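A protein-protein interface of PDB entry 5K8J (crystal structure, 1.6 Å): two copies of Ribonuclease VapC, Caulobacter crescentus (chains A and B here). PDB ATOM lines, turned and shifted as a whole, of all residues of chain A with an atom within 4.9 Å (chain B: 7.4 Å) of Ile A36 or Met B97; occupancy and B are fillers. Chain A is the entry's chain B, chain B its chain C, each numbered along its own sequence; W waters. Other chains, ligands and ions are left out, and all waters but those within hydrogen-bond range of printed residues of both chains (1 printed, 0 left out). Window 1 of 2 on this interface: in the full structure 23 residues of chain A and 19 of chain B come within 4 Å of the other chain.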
ATOM      1  N   SER A  34      12.288  22.017  18.191  1.00  0.00           N
ATOM      2  CA  SER A  34      13.514  22.361  18.916  1.00  0.00           C
ATOM      3  C   SER A  34      14.753  22.055  18.074  1.00  0.00           C
ATOM      4  O   SER A  34      14.821  21.024  17.406  1.00  0.00           O
ATOM      5  CB  SER A  34      13.578  21.552  20.193  1.00  0.00           C
ATOM      6  OG  SER A  34      14.877  21.651  20.734  1.00  0.00           O
ATOM      7  N   ILE A  35      15.753  22.943  18.141  1.00  0.00           N
ATOM      8  CA  ILE A  35      17.048  22.678  17.508  1.00  0.00           C
ATOM      9  C   ILE A  35      17.667  21.401  18.061  1.00  0.00           C
ATOM     10  O   ILE A  35      18.452  20.739  17.375  1.00  0.00           O
ATOM     11  CB  ILE A  35      17.968  23.893  17.699  1.00  0.00           C
ATOM     12  CG1 ILE A  35      19.205  23.812  16.769  1.00  0.00           C
ATOM     13  CG2 ILE A  35      18.443  24.025  19.144  1.00  0.00           C
ATOM     14  CD1 ILE A  35      18.925  24.188  15.390  1.00  0.00           C
ATOM     15  N   ILE A  36      17.368  21.057  19.309  1.00  0.00           N
ATOM     16  CA  ILE A  36      17.883  19.824  19.885  1.00  0.00           C
ATOM     17  C   ILE A  36      17.273  18.629  19.168  1.00  0.00           C
ATOM     18  O   ILE A  36      17.972  17.673  18.812  1.00  0.00           O
ATOM     19  CB  ILE A  36      17.623  19.763  21.411  1.00  0.00           C
ATOM     20  CG1 ILE A  36      18.186  21.005  22.124  1.00  0.00           C
ATOM     21  CG2 ILE A  36      18.207  18.495  21.972  1.00  0.00           C
ATOM     22  CD1 ILE A  36      19.669  21.307  21.836  1.00  0.00           C
ATOM     23  N   SER A  37      15.966  18.677  18.886  1.00  0.00           N
ATOM     24  CA  SER A  37      15.367  17.654  18.042  1.00  0.00           C
ATOM     25  C   SER A  37      15.995  17.631  16.653  1.00  0.00           C
ATOM     26  O   SER A  37      16.180  16.551  16.069  1.00  0.00           O
ATOM     27  CB  SER A  37      13.855  17.877  17.908  1.00  0.00           C
ATOM     28  OG  SER A  37      13.201  17.885  19.160  1.00  0.00           O
ATOM     29  N   ARG A  38      16.274  18.803  16.080  1.00  0.00           N
ATOM     30  CA  ARG A  38      16.964  18.831  14.799  1.00  0.00           C
ATOM     31  C   ARG A  38      18.262  18.030  14.875  1.00  0.00           C
ATOM     32  O   ARG A  38      18.524  17.195  14.012  1.00  0.00           O
ATOM     33  CB  ARG A  38      17.239  20.266  14.329  1.00  0.00           C
ATOM     34  CG  ARG A  38      18.031  20.291  13.046  1.00  0.00           C
ATOM     35  CD  ARG A  38      18.211  21.653  12.381  1.00  0.00           C
ATOM     36  NE  ARG A  38      19.193  21.425  11.321  1.00  0.00           N
ATOM     37  CZ  ARG A  38      20.073  22.306  10.865  1.00  0.00           C
ATOM     38  NH1 ARG A  38      20.060  23.559  11.270  1.00  0.00           N
ATOM     39  NH2 ARG A  38      20.978  21.927   9.966  1.00  0.00           N
ATOM     40  N   VAL A  39      19.060  18.227  15.920  1.00  0.00           N
ATOM     41  CA  VAL A  39      20.314  17.484  16.044  1.00  0.00           C
ATOM     42  C   VAL A  39      20.045  15.986  16.026  1.00  0.00           C
ATOM     43  O   VAL A  39      20.748  15.209  15.361  1.00  0.00           O
ATOM     44  CB  VAL A  39      21.066  17.899  17.317  1.00  0.00           C
ATOM     45  CG1 VAL A  39      22.172  16.914  17.656  1.00  0.00           C
ATOM     46  CG2 VAL A  39      21.649  19.299  17.098  1.00  0.00           C
ATOM     47  N   GLU A  40      19.053  15.556  16.789  1.00  0.00           N
ATOM     48  CA  GLU A  40      18.724  14.141  16.826  1.00  0.00           C
ATOM     49  C   GLU A  40      18.256  13.653  15.466  1.00  0.00           C
ATOM     50  O   GLU A  40      18.659  12.564  15.030  1.00  0.00           O
ATOM     51  CB  GLU A  40      17.679  13.882  17.911  1.00  0.00           C
ATOM     52  CG  GLU A  40      18.134  14.222  19.315  1.00  0.00           C
ATOM     53  CD  GLU A  40      17.081  13.785  20.326  1.00  0.00           C
ATOM     54  OE1 GLU A  40      17.039  12.557  20.595  1.00  0.00           O
ATOM     55  OE2 GLU A  40      16.243  14.642  20.751  1.00  0.00           O
ATOM     56  N   PHE A  71      18.440  26.908  21.212  1.00  0.00           N
ATOM     57  CA  PHE A  71      18.589  26.690  22.649  1.00  0.00           C
ATOM     58  C   PHE A  71      19.479  27.794  23.193  1.00  0.00           C
ATOM     59  O   PHE A  71      20.672  27.837  22.900  1.00  0.00           O
ATOM     60  CB  PHE A  71      19.130  25.296  22.983  1.00  0.00           C
ATOM     61  CG  PHE A  71      18.939  24.954  24.427  1.00  0.00           C
ATOM     62  CD1 PHE A  71      19.849  25.390  25.376  1.00  0.00           C
ATOM     63  CD2 PHE A  71      17.790  24.299  24.860  1.00  0.00           C
ATOM     64  CE1 PHE A  71      19.642  25.136  26.714  1.00  0.00           C
ATOM     65  CE2 PHE A  71      17.574  24.054  26.188  1.00  0.00           C
ATOM     66  CZ  PHE A  71      18.509  24.472  27.130  1.00  0.00           C
ATOM     67  N   VAL A  94      17.940  15.656  27.847  1.00  0.00           N
ATOM     68  CA  VAL A  94      17.407  16.138  26.561  1.00  0.00           C
ATOM     69  C   VAL A  94      15.927  16.481  26.690  1.00  0.00           C
ATOM     70  O   VAL A  94      15.481  17.545  26.240  1.00  0.00           O
ATOM     71  CB  VAL A  94      17.622  15.095  25.449  1.00  0.00           C
ATOM     72  CG1 VAL A  94      16.833  15.506  24.207  1.00  0.00           C
ATOM     73  CG2 VAL A  94      19.095  14.993  25.111  1.00  0.00           C
ATOM     74  N   MET A  97      15.597  19.765  28.414  1.00  0.00           N
ATOM     75  CA  MET A  97      16.013  20.866  27.558  1.00  0.00           C
ATOM     76  C   MET A  97      14.880  21.268  26.615  1.00  0.00           C
ATOM     77  O   MET A  97      14.601  22.451  26.460  1.00  0.00           O
ATOM     78  CB  MET A  97      17.265  20.483  26.753  1.00  0.00           C
ATOM     79  CG  MET A  97      18.535  20.420  27.592  1.00  0.00           C
ATOM     80  SD  MET A  97      20.057  19.875  26.470  1.00  0.00           S
ATOM     81  CE  MET A  97      20.312  21.475  25.548  1.00  0.00           C
ATOM     82  N   ILE A  98      14.258  20.273  25.978  1.00  0.00           N
ATOM     83  CA  ILE A  98      13.189  20.611  25.045  1.00  0.00           C
ATOM     84  C   ILE A  98      11.979  21.171  25.799  1.00  0.00           C
ATOM     85  O   ILE A  98      11.363  22.170  25.384  1.00  0.00           O
ATOM     86  CB  ILE A  98      12.837  19.393  24.178  1.00  0.00           C
ATOM     87  CG1 ILE A  98      14.093  18.921  23.424  1.00  0.00           C
ATOM     88  CG2 ILE A  98      11.708  19.787  23.201  1.00  0.00           C
ATOM     89  CD1 ILE A  98      13.903  17.667  22.631  1.00  0.00           C
ATOM     90  N   GLN A 101      12.447  24.775  26.562  1.00  0.00           N
ATOM     91  CA  GLN A 101      12.173  25.682  25.465  1.00  0.00           C
ATOM     92  C   GLN A 101      10.679  25.931  25.328  1.00  0.00           C
ATOM     93  O   GLN A 101      10.255  27.048  25.040  1.00  0.00           O
ATOM     94  CB  GLN A 101      12.702  25.082  24.178  1.00  0.00           C
ATOM     95  CG  GLN A 101      14.209  24.968  24.177  1.00  0.00           C
ATOM     96  CD  GLN A 101      14.696  24.310  22.917  1.00  0.00           C
ATOM     97  OE1 GLN A 101      14.669  23.101  22.817  1.00  0.00           O
ATOM     98  NE2 GLN A 101      15.155  25.104  21.947  1.00  0.00           N
ATOM     99  N   SER B  34      30.082  26.617  25.945  1.00  0.00           N
ATOM    100  CA  SER B  34      28.886  26.145  25.250  1.00  0.00           C
ATOM    101  C   SER B  34      27.698  26.167  26.196  1.00  0.00           C
ATOM    102  O   SER B  34      27.810  25.763  27.357  1.00  0.00           O
ATOM    103  CB  SER B  34      29.102  24.722  24.753  1.00  0.00           C
ATOM    104  OG  SER B  34      27.890  24.151  24.286  1.00  0.00           O
ATOM    105  N   ILE B  35      26.528  26.581  25.680  1.00  0.00           N
ATOM    106  CA  ILE B  35      25.306  26.449  26.478  1.00  0.00           C
ATOM    107  C   ILE B  35      25.002  24.991  26.789  1.00  0.00           C
ATOM    108  O   ILE B  35      24.316  24.704  27.774  1.00  0.00           O
ATOM    109  CB  ILE B  35      24.111  27.155  25.793  1.00  0.00           C
ATOM    110  CG1 ILE B  35      23.032  27.452  26.832  1.00  0.00           C
ATOM    111  CG2 ILE B  35      23.564  26.319  24.600  1.00  0.00           C
ATOM    112  CD1 ILE B  35      22.053  28.460  26.388  1.00  0.00           C
ATOM    113  N   ILE B  36      25.464  24.055  25.958  1.00  0.00           N
ATOM    114  CA  ILE B  36      25.301  22.638  26.298  1.00  0.00           C
ATOM    115  C   ILE B  36      26.046  22.320  27.586  1.00  0.00           C
ATOM    116  O   ILE B  36      25.518  21.673  28.491  1.00  0.00           O
ATOM    117  CB  ILE B  36      25.785  21.732  25.157  1.00  0.00           C
ATOM    118  CG1 ILE B  36      25.118  22.058  23.814  1.00  0.00           C
ATOM    119  CG2 ILE B  36      25.557  20.264  25.500  1.00  0.00           C
ATOM    120  CD1 ILE B  36      23.608  22.054  23.836  1.00  0.00           C
ATOM    121  N   PHE B  71      22.962  27.494  21.194  1.00  0.00           N
ATOM    122  CA  PHE B  71      23.051  26.404  20.226  1.00  0.00           C
ATOM    123  C   PHE B  71      22.021  26.717  19.147  1.00  0.00           C
ATOM    124  O   PHE B  71      20.811  26.678  19.410  1.00  0.00           O
ATOM    125  CB  PHE B  71      22.818  25.023  20.831  1.00  0.00           C
ATOM    126  CG  PHE B  71      23.202  23.915  19.882  1.00  0.00           C
ATOM    127  CD1 PHE B  71      24.473  23.411  19.885  1.00  0.00           C
ATOM    128  CD2 PHE B  71      22.335  23.490  18.898  1.00  0.00           C
ATOM    129  CE1 PHE B  71      24.868  22.462  18.940  1.00  0.00           C
ATOM    130  CE2 PHE B  71      22.738  22.518  17.970  1.00  0.00           C
ATOM    131  CZ  PHE B  71      24.008  22.037  17.995  1.00  0.00           C
ATOM    132  N   ALA B  75      25.273  26.008  14.338  1.00  0.00           N
ATOM    133  CA  ALA B  75      25.880  24.892  15.039  1.00  0.00           C
ATOM    134  C   ALA B  75      25.281  23.570  14.584  1.00  0.00           C
ATOM    135  O   ALA B  75      26.008  22.586  14.378  1.00  0.00           O
ATOM    136  CB  ALA B  75      25.718  25.059  16.558  1.00  0.00           C
ATOM    137  N   ALA B  76      23.958  23.524  14.396  1.00  0.00           N
ATOM    138  CA  ALA B  76      23.357  22.287  13.930  1.00  0.00           C
ATOM    139  C   ALA B  76      23.811  21.945  12.514  1.00  0.00           C
ATOM    140  O   ALA B  76      23.912  20.757  12.167  1.00  0.00           O
ATOM    141  CB  ALA B  76      21.827  22.360  13.989  1.00  0.00           C
ATOM    142  N   GLU B  78      26.782  22.528  11.364  1.00  0.00           N
ATOM    143  CA  GLU B  78      28.087  21.898  11.561  1.00  0.00           C
ATOM    144  C   GLU B  78      27.940  20.479  12.100  1.00  0.00           C
ATOM    145  O   GLU B  78      28.705  19.584  11.719  1.00  0.00           O
ATOM    146  CB  GLU B  78      28.943  22.742  12.504  1.00  0.00           C
ATOM    147  CG  GLU B  78      29.300  24.121  11.970  1.00  0.00           C
ATOM    148  CD  GLU B  78      30.318  24.143  10.855  1.00  0.00           C
ATOM    149  OE1 GLU B  78      30.605  25.271  10.396  1.00  0.00           O
ATOM    150  OE2 GLU B  78      30.873  23.088  10.468  1.00  0.00           O
ATOM    151  N   TYR B  79      26.986  20.256  13.005  1.00  0.00           N
ATOM    152  CA  TYR B  79      26.749  18.912  13.515  1.00  0.00           C
ATOM    153  C   TYR B  79      26.367  17.959  12.388  1.00  0.00           C
ATOM    154  O   TYR B  79      26.900  16.847  12.285  1.00  0.00           O
ATOM    155  CB  TYR B  79      25.669  18.946  14.598  1.00  0.00           C
ATOM    156  CG  TYR B  79      25.398  17.559  15.105  1.00  0.00           C
ATOM    157  CD1 TYR B  79      26.175  17.021  16.132  1.00  0.00           C
ATOM    158  CD2 TYR B  79      24.410  16.757  14.529  1.00  0.00           C
ATOM    159  CE1 TYR B  79      25.970  15.731  16.552  1.00  0.00           C
ATOM    160  CE2 TYR B  79      24.224  15.448  14.951  1.00  0.00           C
ATOM    161  CZ  TYR B  79      24.988  14.962  15.959  1.00  0.00           C
ATOM    162  OH  TYR B  79      24.811  13.670  16.359  1.00  0.00           O
ATOM    163  N   ILE B  82      29.398  16.955  10.528  1.00  0.00           N
ATOM    164  CA  ILE B  82      30.185  15.966  11.270  1.00  0.00           C
ATOM    165  C   ILE B  82      29.628  14.567  11.049  1.00  0.00           C
ATOM    166  O   ILE B  82      30.359  13.623  10.735  1.00  0.00           O
ATOM    167  CB  ILE B  82      30.203  16.315  12.768  1.00  0.00           C
ATOM    168  CG1 ILE B  82      30.987  17.606  13.007  1.00  0.00           C
ATOM    169  CG2 ILE B  82      30.793  15.162  13.570  1.00  0.00           C
ATOM    170  CD1 ILE B  82      30.868  18.173  14.450  1.00  0.00           C
ATOM    171  N   LYS B  92      28.903  10.027  21.074  1.00  0.00           N
ATOM    172  CA  LYS B  92      29.574  11.300  20.861  1.00  0.00           C
ATOM    173  C   LYS B  92      28.640  12.440  20.466  1.00  0.00           C
ATOM    174  O   LYS B  92      29.120  13.537  20.168  1.00  0.00           O
ATOM    175  CB  LYS B  92      30.665  11.127  19.805  1.00  0.00           C
ATOM    176  CG  LYS B  92      31.717  10.135  20.260  1.00  0.00           C
ATOM    177  CD  LYS B  92      33.099  10.387  19.653  1.00  0.00           C
ATOM    178  CE  LYS B  92      33.172   9.868  18.289  1.00  0.00           C
ATOM    179  NZ  LYS B  92      34.625   9.941  17.791  1.00  0.00           N
ATOM    180  N   VAL B  93      27.324  12.243  20.517  1.00  0.00           N
ATOM    181  CA  VAL B  93      26.405  13.302  20.092  1.00  0.00           C
ATOM    182  C   VAL B  93      26.659  14.592  20.862  1.00  0.00           C
ATOM    183  O   VAL B  93      26.810  15.668  20.279  1.00  0.00           O
ATOM    184  CB  VAL B  93      24.938  12.865  20.241  1.00  0.00           C
ATOM    185  CG1 VAL B  93      24.050  14.064  19.961  1.00  0.00           C
ATOM    186  CG2 VAL B  93      24.594  11.762  19.285  1.00  0.00           C
ATOM    187  N   VAL B  94      26.667  14.521  22.199  1.00  0.00           N
ATOM    188  CA  VAL B  94      26.745  15.744  22.994  1.00  0.00           C
ATOM    189  C   VAL B  94      28.079  16.464  22.809  1.00  0.00           C
ATOM    190  O   VAL B  94      28.121  17.679  22.585  1.00  0.00           O
ATOM    191  CB  VAL B  94      26.475  15.414  24.462  1.00  0.00           C
ATOM    192  CG1 VAL B  94      26.789  16.601  25.336  1.00  0.00           C
ATOM    193  CG2 VAL B  94      25.027  15.013  24.613  1.00  0.00           C
ATOM    194  N   ASP B  95      29.182  15.730  22.830  1.00  0.00           N
ATOM    195  CA  ASP B  95      30.445  16.421  22.632  1.00  0.00           C
ATOM    196  C   ASP B  95      30.595  16.918  21.194  1.00  0.00           C
ATOM    197  O   ASP B  95      31.229  17.955  20.986  1.00  0.00           O
ATOM    198  CB  ASP B  95      31.584  15.534  23.067  1.00  0.00           C
ATOM    199  CG  ASP B  95      31.876  15.680  24.576  1.00  0.00           C
ATOM    200  OD1 ASP B  95      32.268  14.664  25.151  1.00  0.00           O
ATOM    201  OD2 ASP B  95      31.693  16.796  25.179  1.00  0.00           O
ATOM    202  N   ARG B  96      29.963  16.256  20.216  1.00  0.00           N
ATOM    203  CA  ARG B  96      29.965  16.792  18.864  1.00  0.00           C
ATOM    204  C   ARG B  96      29.111  18.050  18.740  1.00  0.00           C
ATOM    205  O   ARG B  96      29.426  18.913  17.915  1.00  0.00           O
ATOM    206  CB  ARG B  96      29.492  15.743  17.868  1.00  0.00           C
ATOM    207  CG  ARG B  96      30.545  14.656  17.603  1.00  0.00           C
ATOM    208  CD  ARG B  96      29.997  13.516  16.837  1.00  0.00           C
ATOM    209  NE  ARG B  96      31.039  12.649  16.299  1.00  0.00           N
ATOM    210  CZ  ARG B  96      30.783  11.669  15.442  1.00  0.00           C
ATOM    211  NH1 ARG B  96      29.529  11.402  15.081  1.00  0.00           N
ATOM    212  NH2 ARG B  96      31.794  10.967  14.934  1.00  0.00           N
ATOM    213  N   MET B  97      28.013  18.174  19.507  1.00  0.00           N
ATOM    214  CA  MET B  97      27.307  19.444  19.549  1.00  0.00           C
ATOM    215  C   MET B  97      28.223  20.597  20.003  1.00  0.00           C
ATOM    216  O   MET B  97      28.184  21.707  19.438  1.00  0.00           O
ATOM    217  CB  MET B  97      26.091  19.355  20.459  1.00  0.00           C
ATOM    218  CG  MET B  97      25.042  18.427  19.879  1.00  0.00           C
ATOM    219  SD  MET B  97      23.556  18.217  21.160  1.00  0.00           S
ATOM    220  CE  MET B  97      23.019  19.473  20.843  1.00  0.00           C
ATOM    221  N   ILE B  98      29.004  20.333  21.062  1.00  0.00           N
ATOM    222  CA  ILE B  98      29.914  21.356  21.568  1.00  0.00           C
ATOM    223  C   ILE B  98      31.002  21.666  20.545  1.00  0.00           C
ATOM    224  O   ILE B  98      31.280  22.825  20.232  1.00  0.00           O
ATOM    225  CB  ILE B  98      30.480  20.926  22.929  1.00  0.00           C
ATOM    226  CG1 ILE B  98      29.342  20.747  23.950  1.00  0.00           C
ATOM    227  CG2 ILE B  98      31.462  21.982  23.435  1.00  0.00           C
ATOM    228  CD1 ILE B  98      29.769  19.992  25.166  1.00  0.00           C
ATOM    229  N   ALA B  99      31.606  20.629  19.952  1.00  0.00           N
ATOM    230  CA  ALA B  99      32.593  20.863  18.910  1.00  0.00           C
ATOM    231  C   ALA B  99      31.991  21.602  17.725  1.00  0.00           C
ATOM    232  O   ALA B  99      32.673  22.391  17.069  1.00  0.00           O
ATOM    233  CB  ALA B  99      33.185  19.533  18.456  1.00  0.00           C
ATOM    234  N   ALA B 100      30.729  21.303  17.394  1.00  0.00           N
ATOM    235  CA  ALA B 100      30.057  21.993  16.303  1.00  0.00           C
ATOM    236  C   ALA B 100      29.962  23.482  16.572  1.00  0.00           C
ATOM    237  O   ALA B 100      30.082  24.272  15.637  1.00  0.00           O
ATOM    238  CB  ALA B 100      28.659  21.433  16.086  1.00  0.00           C
ATOM    239  N   GLN B 101      29.799  23.874  17.830  1.00  0.00           N
ATOM    240  CA  GLN B 101      29.796  25.296  18.156  1.00  0.00           C
ATOM    241  C   GLN B 101      31.175  25.900  17.963  1.00  0.00           C
ATOM    242  O   GLN B 101      31.300  27.012  17.423  1.00  0.00           O
ATOM    243  CB  GLN B 101      29.315  25.517  19.585  1.00  0.00           C
ATOM    244  CG  GLN B 101      27.894  25.073  19.769  1.00  0.00           C
ATOM    245  CD  GLN B 101      27.410  25.339  21.145  1.00  0.00           C
ATOM    246  OE1 GLN B 101      27.677  24.571  22.066  1.00  0.00           O
ATOM    247  NE2 GLN B 101      26.718  26.441  21.304  1.00  0.00           N
ATOM    248  N   ALA B 102      32.235  25.175  18.358  1.00  0.00           N
ATOM    249  CA  ALA B 102      33.574  25.672  18.076  1.00  0.00           C
ATOM    250  C   ALA B 102      33.784  25.850  16.585  1.00  0.00           C
ATOM    251  O   ALA B 102      34.324  26.864  16.134  1.00  0.00           O
ATOM    252  CB  ALA B 102      34.634  24.735  18.651  1.00  0.00           C
ATOM    253  N   LEU B 103      33.377  24.863  15.792  1.00  0.00           N
ATOM    254  CA  LEU B 103      33.531  24.981  14.350  1.00  0.00           C
ATOM    255  C   LEU B 103      32.796  26.193  13.810  1.00  0.00           C
ATOM    256  O   LEU B 103      33.319  26.930  12.959  1.00  0.00           O
ATOM    257  CB  LEU B 103      33.012  23.718  13.665  1.00  0.00           C
ATOM    258  CG  LEU B 103      33.958  22.546  13.662  1.00  0.00           C
ATOM    259  CD1 LEU B 103      33.171  21.287  13.248  1.00  0.00           C
ATOM    260  CD2 LEU B 103      35.123  22.801  12.714  1.00  0.00           C
ATOM    261  N   PHE B 109      38.857  24.179  20.004  1.00  0.00           N
ATOM    262  CA  PHE B 109      38.141  23.380  20.995  1.00  0.00           C
ATOM    263  C   PHE B 109      39.147  22.790  21.983  1.00  0.00           C
ATOM    264  O   PHE B 109      40.083  22.097  21.574  1.00  0.00           O
ATOM    265  CB  PHE B 109      37.358  22.291  20.270  1.00  0.00           C
ATOM    266  CG  PHE B 109      36.526  21.420  21.155  1.00  0.00           C
ATOM    267  CD1 PHE B 109      35.539  21.947  21.956  1.00  0.00           C
ATOM    268  CD2 PHE B 109      36.715  20.051  21.131  1.00  0.00           C
ATOM    269  CE1 PHE B 109      34.763  21.120  22.753  1.00  0.00           C
ATOM    270  CE2 PHE B 109      35.913  19.207  21.912  1.00  0.00           C
ATOM    271  CZ  PHE B 109      34.932  19.762  22.718  1.00  0.00           C
ATOM    272  N   PHE B 117      37.886  13.452  19.006  1.00  0.00           N
ATOM    273  CA  PHE B 117      37.409  14.495  18.107  1.00  0.00           C
ATOM    274  C   PHE B 117      38.278  14.635  16.875  1.00  0.00           C
ATOM    275  O   PHE B 117      38.075  15.560  16.079  1.00  0.00           O
ATOM    276  CB  PHE B 117      37.372  15.844  18.825  1.00  0.00           C
ATOM    277  CG  PHE B 117      36.495  15.870  20.024  1.00  0.00           C
ATOM    278  CD1 PHE B 117      35.193  16.322  19.920  1.00  0.00           C
ATOM    279  CD2 PHE B 117      36.977  15.499  21.258  1.00  0.00           C
ATOM    280  CE1 PHE B 117      34.384  16.371  21.028  1.00  0.00           C
ATOM    281  CE2 PHE B 117      36.180  15.518  22.360  1.00  0.00           C
ATOM    282  CZ  PHE B 117      34.884  15.966  22.259  1.00  0.00           C
ATOM    283  N   ILE B 120      36.823  14.833  13.091  1.00  0.00           N
ATOM    284  CA  ILE B 120      36.015  15.954  12.628  1.00  0.00           C
ATOM    285  C   ILE B 120      36.853  16.804  11.677  1.00  0.00           C
ATOM    286  O   ILE B 120      37.796  17.480  12.133  1.00  0.00           O
ATOM    287  CB  ILE B 120      35.507  16.787  13.803  1.00  0.00           C
ATOM    288  CG1 ILE B 120      34.627  15.898  14.691  1.00  0.00           C
ATOM    289  CG2 ILE B 120      34.783  18.013  13.292  1.00  0.00           C
ATOM    290  CD1 ILE B 120      34.257  16.474  15.999  1.00  0.00           C
HETATM  291  O   HOH W   1      22.228  13.039  16.399  1.00  0.00           O
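Of the 24 printed residues of chain B, 6 touch a printed residue of chain A.
Printed residues of chain B that touch a printed residue of chain A: Ile B35, Ile B36, Phe B71, Ala B76, Tyr B79 and Met B97.
Hydrophobic or aromatic side chains of chain A within 4 Å of the printed part of chain B: Ile A35, Ile A36, Val A39, Phe A71 and Met A97.
Among the printed residues, 10 pairs touch across the chains.
Among the printed residues, no Asp or Glu carboxylate lies within 4 Å of a Lys or Arg side-chain nitrogen of the other chain.
Water W1 bridges OH of Tyr B79 (2.7 Å) and O of Val A39 (2.8 Å).
Ile A35 touches Phe B71, and with the chains exchanged Phe A71 touches Ile B35.
Ile A36 touches Met B97, and with the chains exchanged Met A97 touches Ile B36.
Phe A71 touches its own counterpart, Phe B71.
Of the 10 pairs that touch across the chains among the printed residues, 5 have their exchanged pair printed and touching as well.
O of Phe B71 touches CG2 of Ile A35 (3.6 Å).
CD1 of Ile A35 touches CB of Ala B76, 3.7 Å away.
CD1 of Ile A36 touches CE of Met B97 (3.9 Å).
Ala B76 touches Arg A38.
CE2 of Phe B71 touches CG2 of Val A39, 3.5 Å away.
O of Val A39 touches CE2 of Tyr B79, at 3.5 Å.
Val A39 touches Met B97 (CG1 to CG, 3.9 Å).
Ile B35 touches Phe A71 (CG2 to O, 3.7 Å).
CE of Met A97 touches CD1 of Ile B36, at 3.8 Å.
The side-chain hydroxyl of Ser A34 lies within hydrogen-bond range of the backbone NH of Ile A36, 2.9 Å away.
The backbone NH (N) of Ile B36 sits at hydrogen-bond distance from the side-chain hydroxyl (OG) of Ser B34.
O of Phe A71 sits at hydrogen-bond distance from N of Phe B71 (2.9 Å).
Of chain B, only Met B97 (3.9 Å) comes within 4 Å of Ile A36.
Met B97 touches just these residues of chain A: Ile A36 and Val A39.
Printed residues of chain A within 4 Å of Phe B71: Ile A35, Val A39 and Phe A71.
Of the printed residues of chain A, Tyr B79 touches Val A39 (3.5 Å).
Printed residues of chain B within 4 Å of Met A97: Ile B36 (3.8 Å).
Printed residues of chain B within 4 Å of Ile A35: Phe B71 (3.6 Å) and Ala B76 (3.7 Å).
Val B94 touches none of the printed residues of chain A.
Ser A34 touches none of the printed residues of chain B.
The nearest printed residue of chain A that does not touch Met B97 is Met A97 (5.8 Å).
The nearest printed residue of chain A that does not touch Ala B76 is Val A39 (4.4 Å).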
